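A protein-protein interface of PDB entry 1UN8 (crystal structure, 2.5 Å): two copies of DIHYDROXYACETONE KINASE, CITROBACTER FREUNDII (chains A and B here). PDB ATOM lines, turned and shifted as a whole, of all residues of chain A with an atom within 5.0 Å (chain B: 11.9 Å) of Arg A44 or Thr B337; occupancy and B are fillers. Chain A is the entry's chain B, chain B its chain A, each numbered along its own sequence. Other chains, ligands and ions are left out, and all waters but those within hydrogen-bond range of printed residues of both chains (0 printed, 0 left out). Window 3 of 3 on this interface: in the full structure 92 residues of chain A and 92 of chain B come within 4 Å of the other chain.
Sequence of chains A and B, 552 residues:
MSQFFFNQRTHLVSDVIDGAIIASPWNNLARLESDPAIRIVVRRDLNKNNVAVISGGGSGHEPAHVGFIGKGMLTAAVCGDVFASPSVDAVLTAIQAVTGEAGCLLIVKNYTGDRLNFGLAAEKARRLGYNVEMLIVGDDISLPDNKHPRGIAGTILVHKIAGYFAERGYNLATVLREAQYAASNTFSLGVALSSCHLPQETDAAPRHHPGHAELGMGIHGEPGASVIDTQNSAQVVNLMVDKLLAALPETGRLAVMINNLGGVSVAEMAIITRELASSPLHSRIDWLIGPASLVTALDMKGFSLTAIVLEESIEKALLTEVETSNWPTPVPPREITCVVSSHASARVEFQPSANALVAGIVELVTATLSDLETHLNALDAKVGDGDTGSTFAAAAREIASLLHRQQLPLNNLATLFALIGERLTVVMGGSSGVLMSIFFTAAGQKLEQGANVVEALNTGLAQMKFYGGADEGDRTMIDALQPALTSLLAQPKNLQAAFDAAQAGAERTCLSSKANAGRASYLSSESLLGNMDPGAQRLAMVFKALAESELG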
ATOM      1  N   ASN A  27     -20.891 -21.633 -27.096  1.00  0.00           N
ATOM      2  CA  ASN A  27     -20.012 -21.750 -25.938  1.00  0.00           C
ATOM      3  C   ASN A  27     -20.396 -23.007 -25.187  1.00  0.00           C
ATOM      4  O   ASN A  27     -20.368 -23.047 -23.960  1.00  0.00           O
ATOM      5  CB  ASN A  27     -20.167 -20.530 -25.025  1.00  0.00           C
ATOM      6  CG  ASN A  27     -19.140 -20.504 -23.908  1.00  0.00           C
ATOM      7  OD1 ASN A  27     -18.053 -21.068 -24.042  1.00  0.00           O
ATOM      8  ND2 ASN A  27     -19.466 -19.830 -22.808  1.00  0.00           N
ATOM      9  N   ASN A  28     -20.749 -24.036 -25.949  1.00  0.00           N
ATOM     10  CA  ASN A  28     -21.171 -25.315 -25.396  1.00  0.00           C
ATOM     11  C   ASN A  28     -20.124 -26.397 -25.610  1.00  0.00           C
ATOM     12  O   ASN A  28     -20.435 -27.580 -25.543  1.00  0.00           O
ATOM     13  CB  ASN A  28     -22.469 -25.762 -26.065  1.00  0.00           C
ATOM     14  CG  ASN A  28     -22.298 -26.014 -27.552  1.00  0.00           C
ATOM     15  OD1 ASN A  28     -21.262 -25.694 -28.141  1.00  0.00           O
ATOM     16  ND2 ASN A  28     -23.316 -26.597 -28.169  1.00  0.00           N
ATOM     17  N   LEU A  29     -18.888 -26.004 -25.865  1.00  0.00           N
ATOM     18  CA  LEU A  29     -17.845 -26.986 -26.112  1.00  0.00           C
ATOM     19  C   LEU A  29     -16.787 -26.914 -25.041  1.00  0.00           C
ATOM     20  O   LEU A  29     -16.500 -25.852 -24.516  1.00  0.00           O
ATOM     21  CB  LEU A  29     -17.209 -26.736 -27.481  1.00  0.00           C
ATOM     22  CG  LEU A  29     -18.229 -26.639 -28.619  1.00  0.00           C
ATOM     23  CD1 LEU A  29     -17.571 -26.121 -29.881  1.00  0.00           C
ATOM     24  CD2 LEU A  29     -18.870 -27.998 -28.849  1.00  0.00           C
ATOM     25  N   ALA A  30     -16.200 -28.056 -24.718  1.00  0.00           N
ATOM     26  CA  ALA A  30     -15.164 -28.092 -23.704  1.00  0.00           C
ATOM     27  C   ALA A  30     -14.197 -29.238 -23.971  1.00  0.00           C
ATOM     28  O   ALA A  30     -14.602 -30.312 -24.400  1.00  0.00           O
ATOM     29  CB  ALA A  30     -15.795 -28.249 -22.324  1.00  0.00           C
ATOM     30  N   ARG A  31     -12.914 -29.003 -23.739  1.00  0.00           N
ATOM     31  CA  ARG A  31     -11.943 -30.062 -23.932  1.00  0.00           C
ATOM     32  C   ARG A  31     -12.067 -30.967 -22.715  1.00  0.00           C
ATOM     33  O   ARG A  31     -12.566 -30.552 -21.671  1.00  0.00           O
ATOM     34  CB  ARG A  31     -10.520 -29.501 -24.037  1.00  0.00           C
ATOM     35  CG  ARG A  31     -10.321 -28.599 -25.245  1.00  0.00           C
ATOM     36  CD  ARG A  31      -8.855 -28.338 -25.547  1.00  0.00           C
ATOM     37  NE  ARG A  31      -8.113 -29.566 -25.821  1.00  0.00           N
ATOM     38  CZ  ARG A  31      -6.948 -29.602 -26.463  1.00  0.00           C
ATOM     39  NH1 ARG A  31      -6.411 -28.470 -26.895  1.00  0.00           N
ATOM     40  NH2 ARG A  31      -6.314 -30.757 -26.659  1.00  0.00           N
ATOM     41  N   VAL A  42     -15.945 -32.303 -25.807  1.00  0.00           N
ATOM     42  CA  VAL A  42     -17.251 -32.736 -25.363  1.00  0.00           C
ATOM     43  C   VAL A  42     -18.142 -31.537 -25.113  1.00  0.00           C
ATOM     44  O   VAL A  42     -17.655 -30.409 -24.973  1.00  0.00           O
ATOM     45  CB  VAL A  42     -17.131 -33.573 -24.076  1.00  0.00           C
ATOM     46  CG1 VAL A  42     -16.935 -32.663 -22.854  1.00  0.00           C
ATOM     47  CG2 VAL A  42     -18.348 -34.432 -23.929  1.00  0.00           C
ATOM     48  N   ARG A  43     -19.447 -31.778 -25.072  1.00  0.00           N
ATOM     49  CA  ARG A  43     -20.398 -30.706 -24.825  1.00  0.00           C
ATOM     50  C   ARG A  43     -20.568 -30.459 -23.327  1.00  0.00           C
ATOM     51  O   ARG A  43     -20.429 -31.372 -22.509  1.00  0.00           O
ATOM     52  CB  ARG A  43     -21.744 -31.043 -25.461  1.00  0.00           C
ATOM     53  CG  ARG A  43     -22.267 -32.397 -25.091  1.00  0.00           C
ATOM     54  CD  ARG A  43     -23.439 -32.784 -25.961  1.00  0.00           C
ATOM     55  NE  ARG A  43     -24.625 -32.004 -25.644  1.00  0.00           N
ATOM     56  CZ  ARG A  43     -25.839 -32.265 -26.119  1.00  0.00           C
ATOM     57  NH1 ARG A  43     -26.019 -33.295 -26.939  1.00  0.00           N
ATOM     58  NH2 ARG A  43     -26.868 -31.500 -25.771  1.00  0.00           N
ATOM     59  N   ARG A  44     -20.852 -29.209 -22.972  1.00  0.00           N
ATOM     60  CA  ARG A  44     -21.048 -28.833 -21.578  1.00  0.00           C
ATOM     61  C   ARG A  44     -22.483 -29.162 -21.151  1.00  0.00           C
ATOM     62  O   ARG A  44     -22.809 -29.152 -19.966  1.00  0.00           O
ATOM     63  CB  ARG A  44     -20.737 -27.341 -21.406  1.00  0.00           C
ATOM     64  CG  ARG A  44     -19.259 -27.026 -21.579  1.00  0.00           C
ATOM     65  CD  ARG A  44     -19.031 -25.808 -22.442  1.00  0.00           C
ATOM     66  NE  ARG A  44     -19.439 -24.569 -21.784  1.00  0.00           N
ATOM     67  CZ  ARG A  44     -18.823 -24.047 -20.729  1.00  0.00           C
ATOM     68  NH1 ARG A  44     -17.766 -24.659 -20.211  1.00  0.00           N
ATOM     69  NH2 ARG A  44     -19.261 -22.915 -20.194  1.00  0.00           N
ATOM     70  N   ASP A  45     -23.325 -29.467 -22.140  1.00  0.00           N
ATOM     71  CA  ASP A  45     -24.723 -29.835 -21.922  1.00  0.00           C
ATOM     72  C   ASP A  45     -24.833 -31.307 -21.583  1.00  0.00           C
ATOM     73  O   ASP A  45     -25.859 -31.923 -21.870  1.00  0.00           O
ATOM     74  CB  ASP A  45     -25.535 -29.622 -23.193  1.00  0.00           C
ATOM     75  CG  ASP A  45     -25.720 -28.186 -23.518  1.00  0.00           C
ATOM     76  OD1 ASP A  45     -24.699 -27.467 -23.561  1.00  0.00           O
ATOM     77  OD2 ASP A  45     -26.883 -27.778 -23.730  1.00  0.00           O
ATOM     78  N   LEU A  46     -23.797 -31.885 -20.991  1.00  0.00           N
ATOM     79  CA  LEU A  46     -23.847 -33.306 -20.688  1.00  0.00           C
ATOM     80  C   LEU A  46     -25.080 -33.793 -19.933  1.00  0.00           C
ATOM     81  O   LEU A  46     -25.249 -33.518 -18.750  1.00  0.00           O
ATOM     82  CB  LEU A  46     -22.590 -33.737 -19.938  1.00  0.00           C
ATOM     83  CG  LEU A  46     -21.620 -34.550 -20.795  1.00  0.00           C
ATOM     84  CD1 LEU A  46     -20.662 -35.299 -19.881  1.00  0.00           C
ATOM     85  CD2 LEU A  46     -22.394 -35.544 -21.659  1.00  0.00           C
ATOM     86  N   ALA B 277      -6.049 -15.027 -30.334  1.00  0.00           N
ATOM     87  CA  ALA B 277      -6.512 -15.032 -28.949  1.00  0.00           C
ATOM     88  C   ALA B 277      -5.361 -15.002 -27.958  1.00  0.00           C
ATOM     89  O   ALA B 277      -5.533 -14.627 -26.799  1.00  0.00           O
ATOM     90  CB  ALA B 277      -7.380 -16.262 -28.698  1.00  0.00           C
ATOM     91  N   VAL B 331     -19.100 -12.958 -31.784  1.00  0.00           N
ATOM     92  CA  VAL B 331     -19.061 -13.789 -30.591  1.00  0.00           C
ATOM     93  C   VAL B 331     -17.874 -13.430 -29.709  1.00  0.00           C
ATOM     94  O   VAL B 331     -16.774 -13.201 -30.185  1.00  0.00           O
ATOM     95  CB  VAL B 331     -18.958 -15.290 -30.967  1.00  0.00           C
ATOM     96  CG1 VAL B 331     -18.861 -16.146 -29.706  1.00  0.00           C
ATOM     97  CG2 VAL B 331     -20.160 -15.703 -31.819  1.00  0.00           C
ATOM     98  N   PRO B 332     -18.088 -13.365 -28.400  1.00  0.00           N
ATOM     99  CA  PRO B 332     -16.979 -13.030 -27.506  1.00  0.00           C
ATOM    100  C   PRO B 332     -16.005 -14.202 -27.518  1.00  0.00           C
ATOM    101  O   PRO B 332     -16.432 -15.352 -27.466  1.00  0.00           O
ATOM    102  CB  PRO B 332     -17.659 -12.900 -26.144  1.00  0.00           C
ATOM    103  CG  PRO B 332     -19.072 -12.571 -26.481  1.00  0.00           C
ATOM    104  CD  PRO B 332     -19.357 -13.445 -27.660  1.00  0.00           C
ATOM    105  N   PRO B 333     -14.693 -13.937 -27.599  1.00  0.00           N
ATOM    106  CA  PRO B 333     -13.782 -15.082 -27.601  1.00  0.00           C
ATOM    107  C   PRO B 333     -14.011 -15.882 -26.329  1.00  0.00           C
ATOM    108  O   PRO B 333     -13.811 -15.369 -25.236  1.00  0.00           O
ATOM    109  CB  PRO B 333     -12.407 -14.424 -27.633  1.00  0.00           C
ATOM    110  CG  PRO B 333     -12.634 -13.134 -26.921  1.00  0.00           C
ATOM    111  CD  PRO B 333     -13.944 -12.673 -27.512  1.00  0.00           C
ATOM    112  N   ARG B 334     -14.443 -17.130 -26.473  1.00  0.00           N
ATOM    113  CA  ARG B 334     -14.713 -17.971 -25.314  1.00  0.00           C
ATOM    114  C   ARG B 334     -13.419 -18.458 -24.710  1.00  0.00           C
ATOM    115  O   ARG B 334     -12.412 -18.556 -25.408  1.00  0.00           O
ATOM    116  CB  ARG B 334     -15.537 -19.189 -25.713  1.00  0.00           C
ATOM    117  CG  ARG B 334     -16.643 -18.910 -26.699  1.00  0.00           C
ATOM    118  CD  ARG B 334     -17.648 -17.952 -26.157  1.00  0.00           C
ATOM    119  NE  ARG B 334     -18.871 -17.996 -26.939  1.00  0.00           N
ATOM    120  CZ  ARG B 334     -19.960 -17.290 -26.662  1.00  0.00           C
ATOM    121  NH1 ARG B 334     -19.977 -16.471 -25.611  1.00  0.00           N
ATOM    122  NH2 ARG B 334     -21.033 -17.408 -27.435  1.00  0.00           N
ATOM    123  N   GLU B 335     -13.430 -18.750 -23.412  1.00  0.00           N
ATOM    124  CA  GLU B 335     -12.224 -19.272 -22.785  1.00  0.00           C
ATOM    125  C   GLU B 335     -12.305 -20.788 -22.967  1.00  0.00           C
ATOM    126  O   GLU B 335     -13.387 -21.356 -23.141  1.00  0.00           O
ATOM    127  CB  GLU B 335     -12.142 -18.900 -21.297  1.00  0.00           C
ATOM    128  CG  GLU B 335     -12.963 -19.765 -20.372  1.00  0.00           C
ATOM    129  CD  GLU B 335     -12.733 -19.431 -18.905  1.00  0.00           C
ATOM    130  OE1 GLU B 335     -13.028 -18.283 -18.504  1.00  0.00           O
ATOM    131  OE2 GLU B 335     -12.259 -20.318 -18.155  1.00  0.00           O
ATOM    132  N   ILE B 336     -11.158 -21.440 -22.943  1.00  0.00           N
ATOM    133  CA  ILE B 336     -11.120 -22.871 -23.145  1.00  0.00           C
ATOM    134  C   ILE B 336     -11.246 -23.642 -21.839  1.00  0.00           C
ATOM    135  O   ILE B 336     -10.263 -23.874 -21.139  1.00  0.00           O
ATOM    136  CB  ILE B 336      -9.815 -23.271 -23.858  1.00  0.00           C
ATOM    137  CG1 ILE B 336      -9.446 -22.185 -24.893  1.00  0.00           C
ATOM    138  CG2 ILE B 336      -9.998 -24.655 -24.525  1.00  0.00           C
ATOM    139  CD1 ILE B 336      -8.913 -22.691 -26.191  1.00  0.00           C
ATOM    140  N   THR B 337     -12.461 -24.055 -21.513  1.00  0.00           N
ATOM    141  CA  THR B 337     -12.664 -24.799 -20.286  1.00  0.00           C
ATOM    142  C   THR B 337     -12.264 -26.246 -20.506  1.00  0.00           C
ATOM    143  O   THR B 337     -12.422 -26.789 -21.596  1.00  0.00           O
ATOM    144  CB  THR B 337     -14.129 -24.734 -19.815  1.00  0.00           C
ATOM    145  OG1 THR B 337     -14.971 -25.430 -20.745  1.00  0.00           O
ATOM    146  CG2 THR B 337     -14.577 -23.283 -19.714  1.00  0.00           C
ATOM    147  N   CYS B 338     -11.742 -26.851 -19.448  1.00  0.00           N
ATOM    148  CA  CYS B 338     -11.285 -28.226 -19.474  1.00  0.00           C
ATOM    149  C   CYS B 338     -12.113 -29.050 -18.484  1.00  0.00           C
ATOM    150  O   CYS B 338     -12.013 -28.856 -17.273  1.00  0.00           O
ATOM    151  CB  CYS B 338      -9.810 -28.248 -19.088  1.00  0.00           C
ATOM    152  SG  CYS B 338      -8.918 -29.698 -19.615  1.00  0.00           S
ATOM    153  N   VAL B 339     -12.938 -29.955 -19.005  1.00  0.00           N
ATOM    154  CA  VAL B 339     -13.790 -30.812 -18.176  1.00  0.00           C
ATOM    155  C   VAL B 339     -13.078 -32.067 -17.655  1.00  0.00           C
ATOM    156  O   VAL B 339     -12.199 -32.624 -18.313  1.00  0.00           O
ATOM    157  CB  VAL B 339     -15.020 -31.309 -18.957  1.00  0.00           C
ATOM    158  CG1 VAL B 339     -15.899 -30.138 -19.368  1.00  0.00           C
ATOM    159  CG2 VAL B 339     -14.590 -32.113 -20.174  1.00  0.00           C
ATOM    160  N   VAL B 340     -13.473 -32.506 -16.466  1.00  0.00           N
ATOM    161  CA  VAL B 340     -12.898 -33.693 -15.841  1.00  0.00           C
ATOM    162  C   VAL B 340     -13.970 -34.776 -15.789  1.00  0.00           C
ATOM    163  O   VAL B 340     -15.147 -34.478 -15.559  1.00  0.00           O
ATOM    164  CB  VAL B 340     -12.430 -33.388 -14.401  1.00  0.00           C
ATOM    165  CG1 VAL B 340     -11.702 -34.588 -13.829  1.00  0.00           C
ATOM    166  CG2 VAL B 340     -11.533 -32.162 -14.390  1.00  0.00           C
ATOM    167  N   SER B 341     -13.579 -36.029 -16.011  1.00  0.00           N
ATOM    168  CA  SER B 341     -14.551 -37.119 -15.978  1.00  0.00           C
ATOM    169  C   SER B 341     -14.167 -38.187 -14.972  1.00  0.00           C
ATOM    170  O   SER B 341     -13.053 -38.192 -14.444  1.00  0.00           O
ATOM    171  CB  SER B 341     -14.686 -37.768 -17.353  1.00  0.00           C
ATOM    172  OG  SER B 341     -13.558 -38.574 -17.632  1.00  0.00           O
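N of Val B339 sits at hydrogen-bond distance from O of Arg A31 (2.8 Å).
The backbone carbonyl oxygen of Thr B337 sits at hydrogen-bond distance from the backbone NH of Arg A31, 3.1 Å away.
The side-chain hydroxyl (OG1) of Thr B337 sits at hydrogen-bond distance from the guanidinium group (NH1) of Arg A44.
O of Asn A27 lies within hydrogen-bond range of NE of Arg A44 (2.8 Å).
The backbone NH (N) of Arg A44 lies within hydrogen-bond range of the backbone carbonyl oxygen (O) of Asn A28, 3.1 Å away.
The backbone NH (N) of Ala A30 is in hydrogen-bond range of the backbone carbonyl oxygen (O) of Val A42 (2.8 Å).
Arg B334 touches Asn A27 (NE to CB, 3.4 Å).
Ala A30 touches Thr B337 (CB to OG1, 3.3 Å).
CB of Ala A30 touches CG1 of Val B339 (3.5 Å).
Ile B336 touches Arg A31.
Arg A31 touches Cys B338 (O to CA, 3.4 Å).
CG1 of Val A42 touches CG2 of Val B339 (3.6 Å).
Arg A44 touches one residue of chain B.
No residue of chain B comes within 4 Å of Leu A29.
Val A42 touches one residue of chain B.
No residue of chain B comes within 4 Å of Asp A45.
Printed residues of chain A within 4 Å of Arg B334: Asn A27 (3.4 Å).
Of the printed residues of chain A, Ile B336 touches Arg A31.
Printed residues of chain A within 4 Å of Cys B338: Arg A31.
Pro B332 touches none of the printed residues of chain A.
The nearest residue of chain B that does not touch Arg A44 is Val B339 (5.1 Å).
The nearest printed residue of chain A that does not touch Arg B334 is Asn A28 (6.4 Å).
Hydrophobic or aromatic side chains of chain A that line the printed part of chain B: Ala A30 and Val A42.
Among the printed residues, no Asp or Glu carboxylate lies within 4 Å of a Lys or Arg side-chain nitrogen of the other chain.
No position is printed for both chains.
Of the 9 pairs that touch across the chains among the printed residues, none has its exchanged pair printed and touching as well.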
